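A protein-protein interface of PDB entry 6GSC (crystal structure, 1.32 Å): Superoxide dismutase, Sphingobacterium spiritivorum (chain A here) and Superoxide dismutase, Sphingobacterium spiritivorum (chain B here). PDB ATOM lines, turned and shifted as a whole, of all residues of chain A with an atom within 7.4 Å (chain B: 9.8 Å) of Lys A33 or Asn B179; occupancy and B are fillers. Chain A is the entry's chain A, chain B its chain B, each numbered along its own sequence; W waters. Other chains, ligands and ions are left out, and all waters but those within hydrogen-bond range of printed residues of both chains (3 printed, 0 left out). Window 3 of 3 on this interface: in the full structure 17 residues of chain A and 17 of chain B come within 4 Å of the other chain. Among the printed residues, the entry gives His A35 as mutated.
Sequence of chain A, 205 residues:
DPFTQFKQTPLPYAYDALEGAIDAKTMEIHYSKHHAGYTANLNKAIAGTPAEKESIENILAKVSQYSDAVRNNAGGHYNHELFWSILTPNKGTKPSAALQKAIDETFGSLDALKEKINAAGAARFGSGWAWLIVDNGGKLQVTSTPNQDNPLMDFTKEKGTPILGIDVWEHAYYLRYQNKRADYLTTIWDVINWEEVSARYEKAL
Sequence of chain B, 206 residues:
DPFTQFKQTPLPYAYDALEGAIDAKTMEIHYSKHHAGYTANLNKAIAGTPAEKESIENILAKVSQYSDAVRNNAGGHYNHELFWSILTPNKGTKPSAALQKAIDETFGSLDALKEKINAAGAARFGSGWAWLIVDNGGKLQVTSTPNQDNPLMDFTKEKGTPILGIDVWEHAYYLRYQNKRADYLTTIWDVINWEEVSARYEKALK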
ATOM      1  N   GLN A   8      22.584  -5.060  17.057  1.00  0.00           N
ATOM      2  CA  GLN A   8      22.578  -6.262  16.283  1.00  0.00           C
ATOM      3  C   GLN A   8      23.906  -6.969  16.428  1.00  0.00           C
ATOM      4  O   GLN A   8      24.957  -6.370  16.249  1.00  0.00           O
ATOM      5  CB  GLN A   8      22.384  -6.008  14.783  1.00  0.00           C
ATOM      6  CG  GLN A   8      21.021  -5.505  14.398  1.00  0.00           C
ATOM      7  CD  GLN A   8      20.984  -5.343  12.896  1.00  0.00           C
ATOM      8  OE1 GLN A   8      21.474  -4.342  12.369  1.00  0.00           O
ATOM      9  NE2 GLN A   8      20.476  -6.341  12.214  1.00  0.00           N
ATOM     10  N   TYR A  15      26.060 -12.580   3.554  1.00  0.00           N
ATOM     11  CA  TYR A  15      24.682 -12.533   3.100  1.00  0.00           C
ATOM     12  C   TYR A  15      24.320 -13.630   2.101  1.00  0.00           C
ATOM     13  O   TYR A  15      23.210 -14.079   2.068  1.00  0.00           O
ATOM     14  CB  TYR A  15      24.364 -11.182   2.501  1.00  0.00           C
ATOM     15  CG  TYR A  15      24.343 -10.029   3.450  1.00  0.00           C
ATOM     16  CD1 TYR A  15      23.664 -10.092   4.684  1.00  0.00           C
ATOM     17  CD2 TYR A  15      24.919  -8.810   3.085  1.00  0.00           C
ATOM     18  CE1 TYR A  15      23.596  -8.993   5.503  1.00  0.00           C
ATOM     19  CE2 TYR A  15      24.859  -7.715   3.924  1.00  0.00           C
ATOM     20  CZ  TYR A  15      24.193  -7.822   5.118  1.00  0.00           C
ATOM     21  OH  TYR A  15      24.129  -6.753   5.960  1.00  0.00           O
ATOM     22  N   LYS A  25      19.787 -11.392  -1.434  1.00  0.00           N
ATOM     23  CA  LYS A  25      19.080 -10.137  -1.345  1.00  0.00           C
ATOM     24  C   LYS A  25      18.187 -10.095  -0.089  1.00  0.00           C
ATOM     25  O   LYS A  25      18.188  -9.097   0.647  1.00  0.00           O
ATOM     26  CB  LYS A  25      18.295  -9.855  -2.618  1.00  0.00           C
ATOM     27  CG  LYS A  25      17.610  -8.511  -2.608  1.00  0.00           C
ATOM     28  CD  LYS A  25      18.568  -7.363  -2.360  1.00  0.00           C
ATOM     29  CE  LYS A  25      18.097  -6.091  -3.062  1.00  0.00           C
ATOM     30  NZ  LYS A  25      18.579  -4.795  -2.485  1.00  0.00           N
ATOM     31  N   MET A  27      18.592 -11.925   2.599  1.00  0.00           N
ATOM     32  CA  MET A  27      19.393 -11.860   3.809  1.00  0.00           C
ATOM     33  C   MET A  27      19.811 -10.436   4.045  1.00  0.00           C
ATOM     34  O   MET A  27      19.803  -9.978   5.201  1.00  0.00           O
ATOM     35  CB  MET A  27      20.608 -12.780   3.687  1.00  0.00           C
ATOM     36  CG  MET A  27      20.277 -14.263   3.726  1.00  0.00           C
ATOM     37  SD  MET A  27      19.492 -14.793   5.258  1.00  0.00           S
ATOM     38  CE  MET A  27      20.738 -14.366   6.486  1.00  0.00           C
ATOM     39  N   GLU A  28      20.256  -9.714   3.046  1.00  0.00           N
ATOM     40  CA  GLU A  28      20.743  -8.379   3.237  1.00  0.00           C
ATOM     41  C   GLU A  28      19.646  -7.437   3.708  1.00  0.00           C
ATOM     42  O   GLU A  28      19.840  -6.638   4.640  1.00  0.00           O
ATOM     43  CB  GLU A  28      21.364  -7.910   1.915  1.00  0.00           C
ATOM     44  CG  GLU A  28      21.887  -6.483   2.022  1.00  0.00           C
ATOM     45  CD  GLU A  28      22.863  -6.120   0.929  1.00  0.00           C
ATOM     46  OE1 GLU A  28      22.732  -6.661  -0.208  1.00  0.00           O
ATOM     47  OE2 GLU A  28      23.742  -5.273   1.217  1.00  0.00           O
ATOM     48  N   ILE A  29      18.484  -7.475   3.075  1.00  0.00           N
ATOM     49  CA  ILE A  29      17.403  -6.593   3.474  1.00  0.00           C
ATOM     50  C   ILE A  29      16.875  -6.983   4.863  1.00  0.00           C
ATOM     51  O   ILE A  29      16.613  -6.143   5.707  1.00  0.00           O
ATOM     52  CB  ILE A  29      16.276  -6.636   2.441  1.00  0.00           C
ATOM     53  CG1 ILE A  29      16.790  -6.164   1.065  1.00  0.00           C
ATOM     54  CG2 ILE A  29      15.030  -5.858   2.919  1.00  0.00           C
ATOM     55  CD1 ILE A  29      15.824  -6.328  -0.059  1.00  0.00           C
ATOM     56  N   HIS A  30      16.686  -8.270   5.040  1.00  0.00           N
ATOM     57  CA  HIS A  30      16.140  -8.780   6.289  1.00  0.00           C
ATOM     58  C   HIS A  30      16.987  -8.349   7.471  1.00  0.00           C
ATOM     59  O   HIS A  30      16.515  -7.948   8.536  1.00  0.00           O
ATOM     60  CB  HIS A  30      16.005 -10.279   6.187  1.00  0.00           C
ATOM     61  CG  HIS A  30      15.074 -10.882   7.170  1.00  0.00           C
ATOM     62  ND1 HIS A  30      14.821 -12.217   7.185  1.00  0.00           N
ATOM     63  CD2 HIS A  30      14.336 -10.333   8.161  1.00  0.00           C
ATOM     64  CE1 HIS A  30      13.922 -12.490   8.123  1.00  0.00           C
ATOM     65  NE2 HIS A  30      13.598 -11.352   8.712  1.00  0.00           N
ATOM     66  N   TYR A  31      18.295  -8.460   7.320  1.00  0.00           N
ATOM     67  CA  TYR A  31      19.235  -8.080   8.381  1.00  0.00           C
ATOM     68  C   TYR A  31      19.373  -6.556   8.471  1.00  0.00           C
ATOM     69  O   TYR A  31      19.252  -5.981   9.573  1.00  0.00           O
ATOM     70  CB  TYR A  31      20.601  -8.742   8.138  1.00  0.00           C
ATOM     71  CG  TYR A  31      21.580  -8.455   9.254  1.00  0.00           C
ATOM     72  CD1 TYR A  31      21.628  -9.262  10.370  1.00  0.00           C
ATOM     73  CD2 TYR A  31      22.467  -7.411   9.158  1.00  0.00           C
ATOM     74  CE1 TYR A  31      22.521  -8.993  11.410  1.00  0.00           C
ATOM     75  CE2 TYR A  31      23.394  -7.167  10.175  1.00  0.00           C
ATOM     76  CZ  TYR A  31      23.376  -7.952  11.283  1.00  0.00           C
ATOM     77  OH  TYR A  31      24.299  -7.704  12.302  1.00  0.00           O
ATOM     78  N   SER A  32      19.678  -5.912   7.360  1.00  0.00           N
ATOM     79  CA  SER A  32      20.129  -4.517   7.401  1.00  0.00           C
ATOM     80  C   SER A  32      19.012  -3.511   7.382  1.00  0.00           C
ATOM     81  O   SER A  32      19.242  -2.335   7.655  1.00  0.00           O
ATOM     82  CB  SER A  32      21.100  -4.210   6.248  1.00  0.00           C
ATOM     83  OG  SER A  32      20.442  -4.067   5.012  1.00  0.00           O
ATOM     84  N   LYS A  33      17.800  -3.940   7.057  1.00  0.00           N
ATOM     85  CA  LYS A  33      16.653  -3.093   7.032  1.00  0.00           C
ATOM     86  C   LYS A  33      15.650  -3.536   8.059  1.00  0.00           C
ATOM     87  O   LYS A  33      15.365  -2.791   8.988  1.00  0.00           O
ATOM     88  CB  LYS A  33      16.022  -2.993   5.636  1.00  0.00           C
ATOM     89  CG  LYS A  33      16.956  -2.529   4.549  1.00  0.00           C
ATOM     90  CD  LYS A  33      17.359  -1.090   4.680  1.00  0.00           C
ATOM     91  CE  LYS A  33      18.279  -0.725   3.520  1.00  0.00           C
ATOM     92  NZ  LYS A  33      18.234   0.752   3.382  1.00  0.00           N
ATOM     93  N   HIS A  34      15.108  -4.736   7.947  1.00  0.00           N
ATOM     94  CA  HIS A  34      14.043  -5.103   8.899  1.00  0.00           C
ATOM     95  C   HIS A  34      14.614  -5.230  10.317  1.00  0.00           C
ATOM     96  O   HIS A  34      14.125  -4.575  11.244  1.00  0.00           O
ATOM     97  CB  HIS A  34      13.340  -6.387   8.485  1.00  0.00           C
ATOM     98  CG  HIS A  34      12.609  -6.271   7.187  1.00  0.00           C
ATOM     99  ND1 HIS A  34      11.462  -5.538   7.059  1.00  0.00           N
ATOM    100  CD2 HIS A  34      12.825  -6.828   5.968  1.00  0.00           C
ATOM    101  CE1 HIS A  34      11.012  -5.615   5.815  1.00  0.00           C
ATOM    102  NE2 HIS A  34      11.818  -6.396   5.138  1.00  0.00           N
ATOM    103  N   HIS A  35      15.624  -6.076  10.535  1.00  0.00           N
ATOM    104  CA  HIS A  35      16.125  -6.257  11.886  1.00  0.00           C
ATOM    105  C   HIS A  35      16.718  -4.969  12.363  1.00  0.00           C
ATOM    106  O   HIS A  35      16.436  -4.528  13.504  1.00  0.00           O
ATOM    107  CB  HIS A  35      17.114  -7.392  11.955  1.00  0.00           C
ATOM    108  CG  HIS A  35      17.618  -7.634  13.330  1.00  0.00           C
ATOM    109  ND1 HIS A  35      18.681  -8.469  13.567  1.00  0.00           N
ATOM    110  CD2 HIS A  35      17.194  -7.206  14.548  1.00  0.00           C
ATOM    111  CE1 HIS A  35      18.926  -8.515  14.856  1.00  0.00           C
ATOM    112  NE2 HIS A  35      18.031  -7.769  15.470  1.00  0.00           N
ATOM    113  N   ALA A  36      17.573  -4.324  11.586  1.00  0.00           N
ATOM    114  CA  ALA A  36      18.176  -3.062  12.017  1.00  0.00           C
ATOM    115  C   ALA A  36      17.121  -2.080  12.461  1.00  0.00           C
ATOM    116  O   ALA A  36      17.313  -1.353  13.445  1.00  0.00           O
ATOM    117  CB  ALA A  36      19.040  -2.470  10.905  1.00  0.00           C
ATOM    118  N   GLY A  37      15.984  -2.029  11.782  1.00  0.00           N
ATOM    119  CA  GLY A  37      14.913  -1.138  12.151  1.00  0.00           C
ATOM    120  C   GLY A  37      14.318  -1.469  13.521  1.00  0.00           C
ATOM    121  O   GLY A  37      14.050  -0.571  14.335  1.00  0.00           O
ATOM    122  N   TYR A  38      14.091  -2.739  13.792  1.00  0.00           N
ATOM    123  CA  TYR A  38      13.596  -3.133  15.105  1.00  0.00           C
ATOM    124  C   TYR A  38      14.554  -2.751  16.196  1.00  0.00           C
ATOM    125  O   TYR A  38      14.139  -2.237  17.234  1.00  0.00           O
ATOM    126  CB  TYR A  38      13.340  -4.636  15.165  1.00  0.00           C
ATOM    127  CG  TYR A  38      12.243  -5.105  14.210  1.00  0.00           C
ATOM    128  CD1 TYR A  38      11.032  -4.481  14.131  1.00  0.00           C
ATOM    129  CD2 TYR A  38      12.436  -6.193  13.388  1.00  0.00           C
ATOM    130  CE1 TYR A  38      10.058  -4.932  13.246  1.00  0.00           C
ATOM    131  CE2 TYR A  38      11.448  -6.643  12.527  1.00  0.00           C
ATOM    132  CZ  TYR A  38      10.301  -6.009  12.478  1.00  0.00           C
ATOM    133  OH  TYR A  38       9.309  -6.466  11.600  1.00  0.00           O
ATOM    134  N   THR A  39      15.857  -2.969  15.976  1.00  0.00           N
ATOM    135  CA  THR A  39      16.855  -2.668  17.033  1.00  0.00           C
ATOM    136  C   THR A  39      16.855  -1.176  17.312  1.00  0.00           C
ATOM    137  O   THR A  39      16.840  -0.729  18.462  1.00  0.00           O
ATOM    138  CB  THR A  39      18.227  -3.151  16.577  1.00  0.00           C
ATOM    139  OG1 THR A  39      18.128  -4.537  16.287  1.00  0.00           O
ATOM    140  CG2 THR A  39      19.232  -2.944  17.711  1.00  0.00           C
ATOM    141  N   HIS A 171       8.314 -11.159   4.186  1.00  0.00           N
ATOM    142  CA  HIS A 171       9.654 -10.651   3.825  1.00  0.00           C
ATOM    143  C   HIS A 171      10.741 -11.708   3.982  1.00  0.00           C
ATOM    144  O   HIS A 171      11.814 -11.553   3.399  1.00  0.00           O
ATOM    145  CB  HIS A 171      10.037  -9.372   4.571  1.00  0.00           C
ATOM    146  CG  HIS A 171      10.143  -9.520   6.080  1.00  0.00           C
ATOM    147  ND1 HIS A 171       9.405  -8.733   6.939  1.00  0.00           N
ATOM    148  CD2 HIS A 171      10.975 -10.238   6.879  1.00  0.00           C
ATOM    149  CE1 HIS A 171       9.761  -8.989   8.200  1.00  0.00           C
ATOM    150  NE2 HIS A 171      10.702  -9.892   8.197  1.00  0.00           N
ATOM    151  N   GLY B 121      -1.461   3.156   6.430  1.00  0.00           N
ATOM    152  CA  GLY B 121      -0.831   2.001   5.857  1.00  0.00           C
ATOM    153  C   GLY B 121       0.530   1.729   6.445  1.00  0.00           C
ATOM    154  O   GLY B 121       0.871   0.572   6.719  1.00  0.00           O
ATOM    155  N   ALA B 122       1.324   2.775   6.635  1.00  0.00           N
ATOM    156  CA  ALA B 122       2.649   2.603   7.178  1.00  0.00           C
ATOM    157  C   ALA B 122       2.597   2.158   8.630  1.00  0.00           C
ATOM    158  O   ALA B 122       3.490   1.424   9.086  1.00  0.00           O
ATOM    159  CB  ALA B 122       3.436   3.922   7.093  1.00  0.00           C
ATOM    160  N   VAL B 168      -1.575  -3.902   2.389  1.00  0.00           N
ATOM    161  CA  VAL B 168      -0.210  -3.748   2.835  1.00  0.00           C
ATOM    162  C   VAL B 168       0.364  -5.017   3.393  1.00  0.00           C
ATOM    163  O   VAL B 168       1.404  -4.984   4.121  1.00  0.00           O
ATOM    164  CB  VAL B 168      -0.002  -2.549   3.779  1.00  0.00           C
ATOM    165  CG1 VAL B 168      -0.299  -1.232   3.090  1.00  0.00           C
ATOM    166  CG2 VAL B 168      -0.793  -2.649   5.095  1.00  0.00           C
ATOM    167  N   GLU B 170       2.916  -7.856   2.831  1.00  0.00           N
ATOM    168  CA  GLU B 170       4.171  -7.816   2.083  1.00  0.00           C
ATOM    169  C   GLU B 170       4.009  -8.441   0.730  1.00  0.00           C
ATOM    170  O   GLU B 170       4.667  -7.979  -0.198  1.00  0.00           O
ATOM    171  CB  GLU B 170       5.314  -8.368   2.912  1.00  0.00           C
ATOM    172  CG  GLU B 170       5.718  -7.430   4.057  1.00  0.00           C
ATOM    173  CD  GLU B 170       6.703  -7.997   5.097  1.00  0.00           C
ATOM    174  OE1 GLU B 170       6.642  -9.192   5.384  1.00  0.00           O
ATOM    175  OE2 GLU B 170       7.481  -7.143   5.599  1.00  0.00           O
ATOM    176  N   TYR B 173       3.642  -5.984  -2.224  1.00  0.00           N
ATOM    177  CA  TYR B 173       4.650  -5.040  -2.641  1.00  0.00           C
ATOM    178  C   TYR B 173       6.065  -5.536  -2.578  1.00  0.00           C
ATOM    179  O   TYR B 173       6.968  -4.799  -3.005  1.00  0.00           O
ATOM    180  CB  TYR B 173       4.524  -3.752  -1.836  1.00  0.00           C
ATOM    181  CG  TYR B 173       4.751  -3.871  -0.329  1.00  0.00           C
ATOM    182  CD1 TYR B 173       6.026  -3.832   0.218  1.00  0.00           C
ATOM    183  CD2 TYR B 173       3.675  -3.983   0.544  1.00  0.00           C
ATOM    184  CE1 TYR B 173       6.235  -3.907   1.597  1.00  0.00           C
ATOM    185  CE2 TYR B 173       3.873  -4.014   1.921  1.00  0.00           C
ATOM    186  CZ  TYR B 173       5.158  -4.001   2.426  1.00  0.00           C
ATOM    187  OH  TYR B 173       5.315  -4.052   3.820  1.00  0.00           O
ATOM    188  N   TYR B 174       6.343  -6.729  -2.075  1.00  0.00           N
ATOM    189  CA  TYR B 174       7.704  -7.048  -1.762  1.00  0.00           C
ATOM    190  C   TYR B 174       8.561  -7.261  -3.011  1.00  0.00           C
ATOM    191  O   TYR B 174       9.740  -6.953  -2.987  1.00  0.00           O
ATOM    192  CB  TYR B 174       7.801  -8.258  -0.803  1.00  0.00           C
ATOM    193  CG  TYR B 174       8.946  -8.117   0.159  1.00  0.00           C
ATOM    194  CD1 TYR B 174      10.153  -8.703  -0.083  1.00  0.00           C
ATOM    195  CD2 TYR B 174       8.856  -7.234   1.215  1.00  0.00           C
ATOM    196  CE1 TYR B 174      11.260  -8.540   0.761  1.00  0.00           C
ATOM    197  CE2 TYR B 174       9.939  -7.057   2.046  1.00  0.00           C
ATOM    198  CZ  TYR B 174      11.127  -7.660   1.798  1.00  0.00           C
ATOM    199  OH  TYR B 174      12.174  -7.395   2.664  1.00  0.00           O
ATOM    200  N   LEU B 175       8.009  -7.850  -4.086  1.00  0.00           N
ATOM    201  CA  LEU B 175       8.844  -8.145  -5.266  1.00  0.00           C
ATOM    202  C   LEU B 175       9.400  -6.863  -5.856  1.00  0.00           C
ATOM    203  O   LEU B 175      10.556  -6.839  -6.265  1.00  0.00           O
ATOM    204  CB  LEU B 175       8.084  -8.937  -6.327  1.00  0.00           C
ATOM    205  CG  LEU B 175       7.713 -10.357  -5.917  1.00  0.00           C
ATOM    206  CD1 LEU B 175       7.040 -11.012  -7.118  1.00  0.00           C
ATOM    207  CD2 LEU B 175       8.897 -11.162  -5.465  1.00  0.00           C
ATOM    208  N   ARG B 176       8.620  -5.813  -5.886  1.00  0.00           N
ATOM    209  CA  ARG B 176       9.050  -4.561  -6.505  1.00  0.00           C
ATOM    210  C   ARG B 176       9.703  -3.603  -5.504  1.00  0.00           C
ATOM    211  O   ARG B 176      10.609  -2.870  -5.848  1.00  0.00           O
ATOM    212  CB  ARG B 176       7.863  -3.890  -7.180  1.00  0.00           C
ATOM    213  CG  ARG B 176       8.188  -2.534  -7.784  1.00  0.00           C
ATOM    214  CD  ARG B 176       7.329  -2.434  -9.038  1.00  0.00           C
ATOM    215  NE  ARG B 176       7.061  -1.109  -9.507  1.00  0.00           N
ATOM    216  CZ  ARG B 176       6.518  -0.876 -10.694  1.00  0.00           C
ATOM    217  NH1 ARG B 176       6.338  -1.872 -11.555  1.00  0.00           N
ATOM    218  NH2 ARG B 176       6.274   0.357 -11.043  1.00  0.00           N
ATOM    219  N   TYR B 177       9.194  -3.551  -4.270  1.00  0.00           N
ATOM    220  CA  TYR B 177       9.566  -2.498  -3.313  1.00  0.00           C
ATOM    221  C   TYR B 177      10.309  -3.042  -2.103  1.00  0.00           C
ATOM    222  O   TYR B 177      10.856  -2.250  -1.326  1.00  0.00           O
ATOM    223  CB  TYR B 177       8.320  -1.811  -2.804  1.00  0.00           C
ATOM    224  CG  TYR B 177       7.534  -1.074  -3.872  1.00  0.00           C
ATOM    225  CD1 TYR B 177       7.866   0.225  -4.208  1.00  0.00           C
ATOM    226  CD2 TYR B 177       6.503  -1.682  -4.531  1.00  0.00           C
ATOM    227  CE1 TYR B 177       7.160   0.901  -5.171  1.00  0.00           C
ATOM    228  CE2 TYR B 177       5.819  -1.024  -5.512  1.00  0.00           C
ATOM    229  CZ  TYR B 177       6.148   0.263  -5.819  1.00  0.00           C
ATOM    230  OH  TYR B 177       5.428   0.917  -6.830  1.00  0.00           O
ATOM    231  N   GLN B 178      10.362  -4.357  -1.951  1.00  0.00           N
ATOM    232  CA  GLN B 178      10.931  -4.967  -0.755  1.00  0.00           C
ATOM    233  C   GLN B 178      10.411  -4.266   0.506  1.00  0.00           C
ATOM    234  O   GLN B 178       9.188  -4.129   0.659  1.00  0.00           O
ATOM    235  CB  GLN B 178      12.412  -5.074  -0.840  1.00  0.00           C
ATOM    236  CG  GLN B 178      12.873  -5.908  -2.036  1.00  0.00           C
ATOM    237  CD  GLN B 178      13.004  -5.148  -3.302  1.00  0.00           C
ATOM    238  OE1 GLN B 178      13.641  -4.097  -3.351  1.00  0.00           O
ATOM    239  NE2 GLN B 178      12.345  -5.628  -4.343  1.00  0.00           N
ATOM    240  N   ASN B 179      11.282  -3.824   1.400  1.00  0.00           N
ATOM    241  CA  ASN B 179      10.873  -3.246   2.654  1.00  0.00           C
ATOM    242  C   ASN B 179      10.282  -1.848   2.527  1.00  0.00           C
ATOM    243  O   ASN B 179       9.774  -1.298   3.502  1.00  0.00           O
ATOM    244  CB  ASN B 179      12.100  -3.122   3.543  1.00  0.00           C
ATOM    245  CG  ASN B 179      13.184  -2.262   2.923  1.00  0.00           C
ATOM    246  OD1 ASN B 179      13.753  -2.603   1.885  1.00  0.00           O
ATOM    247  ND2 ASN B 179      13.474  -1.114   3.566  1.00  0.00           N
ATOM    248  N   LYS B 180      10.269  -1.256   1.341  1.00  0.00           N
ATOM    249  CA  LYS B 180       9.889   0.130   1.185  1.00  0.00           C
ATOM    250  C   LYS B 180       8.399   0.256   0.948  1.00  0.00           C
ATOM    251  O   LYS B 180       7.912   0.701  -0.105  1.00  0.00           O
ATOM    252  CB  LYS B 180      10.653   0.732   0.025  1.00  0.00           C
ATOM    253  CG  LYS B 180      12.157   0.719   0.276  1.00  0.00           C
ATOM    254  CD  LYS B 180      12.964   1.313  -0.881  1.00  0.00           C
ATOM    255  CE  LYS B 180      12.741   0.618  -2.220  1.00  0.00           C
ATOM    256  NZ  LYS B 180      13.058  -0.818  -2.207  1.00  0.00           N
ATOM    257  N   ARG B 181       7.643  -0.086   1.961  1.00  0.00           N
ATOM    258  CA  ARG B 181       6.200   0.001   1.911  1.00  0.00           C
ATOM    259  C   ARG B 181       5.779   1.413   1.636  1.00  0.00           C
ATOM    260  O   ARG B 181       4.778   1.635   0.981  1.00  0.00           O
ATOM    261  CB  ARG B 181       5.594  -0.451   3.233  1.00  0.00           C
ATOM    262  CG  ARG B 181       4.081  -0.511   3.203  1.00  0.00           C
ATOM    263  CD  ARG B 181       3.477  -0.710   4.585  1.00  0.00           C
ATOM    264  NE  ARG B 181       3.685  -2.046   5.098  1.00  0.00           N
ATOM    265  CZ  ARG B 181       3.144  -2.482   6.247  1.00  0.00           C
ATOM    266  NH1 ARG B 181       2.338  -1.715   6.967  1.00  0.00           N
ATOM    267  NH2 ARG B 181       3.387  -3.733   6.647  1.00  0.00           N
ATOM    268  N   ALA B 182       6.438   2.396   2.216  1.00  0.00           N
ATOM    269  CA  ALA B 182       6.058   3.776   1.971  1.00  0.00           C
ATOM    270  C   ALA B 182       6.132   4.156   0.485  1.00  0.00           C
ATOM    271  O   ALA B 182       5.317   4.953   0.035  1.00  0.00           O
ATOM    272  CB  ALA B 182       6.928   4.719   2.804  1.00  0.00           C
ATOM    273  N   ASP B 183       7.106   3.643  -0.231  1.00  0.00           N
ATOM    274  CA  ASP B 183       7.241   3.937  -1.656  1.00  0.00           C
ATOM    275  C   ASP B 183       6.100   3.294  -2.422  1.00  0.00           C
ATOM    276  O   ASP B 183       5.541   3.870  -3.368  1.00  0.00           O
ATOM    277  CB  ASP B 183       8.554   3.457  -2.209  1.00  0.00           C
ATOM    278  CG  ASP B 183       9.747   4.299  -1.780  1.00  0.00           C
ATOM    279  OD1 ASP B 183       9.594   5.351  -1.167  1.00  0.00           O
ATOM    280  OD2 ASP B 183      10.861   3.883  -2.127  1.00  0.00           O
ATOM    281  N   TYR B 184       5.737   2.069  -2.040  1.00  0.00           N
ATOM    282  CA  TYR B 184       4.534   1.424  -2.576  1.00  0.00           C
ATOM    283  C   TYR B 184       3.300   2.254  -2.383  1.00  0.00           C
ATOM    284  O   TYR B 184       2.529   2.492  -3.355  1.00  0.00           O
ATOM    285  CB  TYR B 184       4.342   0.057  -1.967  1.00  0.00           C
ATOM    286  CG  TYR B 184       3.018  -0.628  -2.110  1.00  0.00           C
ATOM    287  CD1 TYR B 184       2.552  -1.051  -3.325  1.00  0.00           C
ATOM    288  CD2 TYR B 184       2.256  -0.850  -0.983  1.00  0.00           C
ATOM    289  CE1 TYR B 184       1.337  -1.717  -3.416  1.00  0.00           C
ATOM    290  CE2 TYR B 184       1.073  -1.512  -1.051  1.00  0.00           C
ATOM    291  CZ  TYR B 184       0.617  -1.941  -2.283  1.00  0.00           C
ATOM    292  OH  TYR B 184      -0.576  -2.636  -2.377  1.00  0.00           O
ATOM    293  N   LEU B 185       3.103   2.734  -1.168  1.00  0.00           N
ATOM    294  CA  LEU B 185       1.927   3.549  -0.865  1.00  0.00           C
ATOM    295  C   LEU B 185       1.933   4.846  -1.635  1.00  0.00           C
ATOM    296  O   LEU B 185       0.854   5.264  -2.142  1.00  0.00           O
ATOM    297  CB  LEU B 185       1.840   3.792   0.635  1.00  0.00           C
ATOM    298  CG  LEU B 185       1.413   2.540   1.418  1.00  0.00           C
ATOM    299  CD1 LEU B 185       1.669   2.705   2.920  1.00  0.00           C
ATOM    300  CD2 LEU B 185      -0.058   2.243   1.187  1.00  0.00           C
HETATM  301  O   HOH W   1      15.336   0.935   2.431  1.00  0.00           O
HETATM  302  O   HOH W   2      15.865  -3.288  -2.069  1.00  0.00           O
HETATM  303  O   HOH W   3      13.765  -9.422   3.701  1.00  0.00           O
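A ring nitrogen (ND1) of His A171 sits at hydrogen-bond distance from the side-chain carboxylate (OE2) of Glu B170, at 2.8 Å.
A ring nitrogen (NE2) of His A34 is in hydrogen-bond range of the side-chain hydroxyl (OH) of Tyr B174.
The side-chain amide nitrogen (NE2) of Gln B178 sits close to the backbone carbonyl oxygen (O) of Tyr B174 (3.2 Å).
The backbone NH of His A34 sits at hydrogen-bond distance from the backbone carbonyl oxygen of Ile A29 (3.0 Å).
The backbone carbonyl oxygen of Leu B175 is in hydrogen-bond range of the side-chain amide nitrogen of Gln B178.
Among the printed residues, merely in contact across the chains: Ile A29 with Tyr B174, Ile A29 with Gln B178, Ile A29 with Asn B179, Lys A33 with Asn B179, His A34 with Glu B170, His A34 with Asn B179 and His A171 with Tyr B174.
Gln A8 touches none of the printed residues of chain B.
Of chain B, only Tyr B174 (3.3 Å), Gln B178 (3.6 Å) and Asn B179 (3.6 Å) come within 4 Å of Ile A29.
No residue of chain B comes within 4 Å of Ser A32.
Lys A33 touches just one residue of chain B: Asn B179.
Of chain B, only Glu B170, Tyr B174 and Asn B179 come within 4 Å of His A34.
Of the printed residues of chain B, His A171 touches Glu B170 and Tyr B174.
Of the printed residues of chain A, Glu B170 touches His A34 (3.9 Å) and His A171 (2.8 Å).
Of the printed residues of chain A, Tyr B174 touches Ile A29 (3.3 Å), His A34 (2.7 Å) and His A171 (3.4 Å).
Printed residues of chain A within 4 Å of Gln B178: Ile A29.
Asn B179 touches three residues of chain A.
The nearest residue of chain B that does not touch Lys A33 is Tyr B174 (6.6 Å).
The nearest residue of chain A that does not touch Asn B179 is His A171 (6.5 Å).
Of the 17 printed residues of chain A, 4 touch a printed residue of chain B.
Printed residues of chain A that touch a printed residue of chain B: Ile A29, Lys A33, His A34 and His A171.
Of the 17 printed residues of chain B, 4 touch a printed residue of chain A.
Printed residues of chain B that touch a printed residue of chain A: Glu B170, Tyr B174, Gln B178 and Asn B179.
Hydrophobic or aromatic side chains of chain B within 4 Å of the printed part of chain A: Tyr B174.
Water W2 lies within hydrogen-bond range of OE1 of Gln B178 (2.7 Å) and NZ of Lys A25 (3.1 Å).
Water W3 lies within hydrogen-bond range of OH of Tyr B174, O of His A171 and N of His A30.
Water W1 lies within hydrogen-bond range of ND2 of Asn B179 (3.0 Å) and NZ of Lys A33 (3.1 Å).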
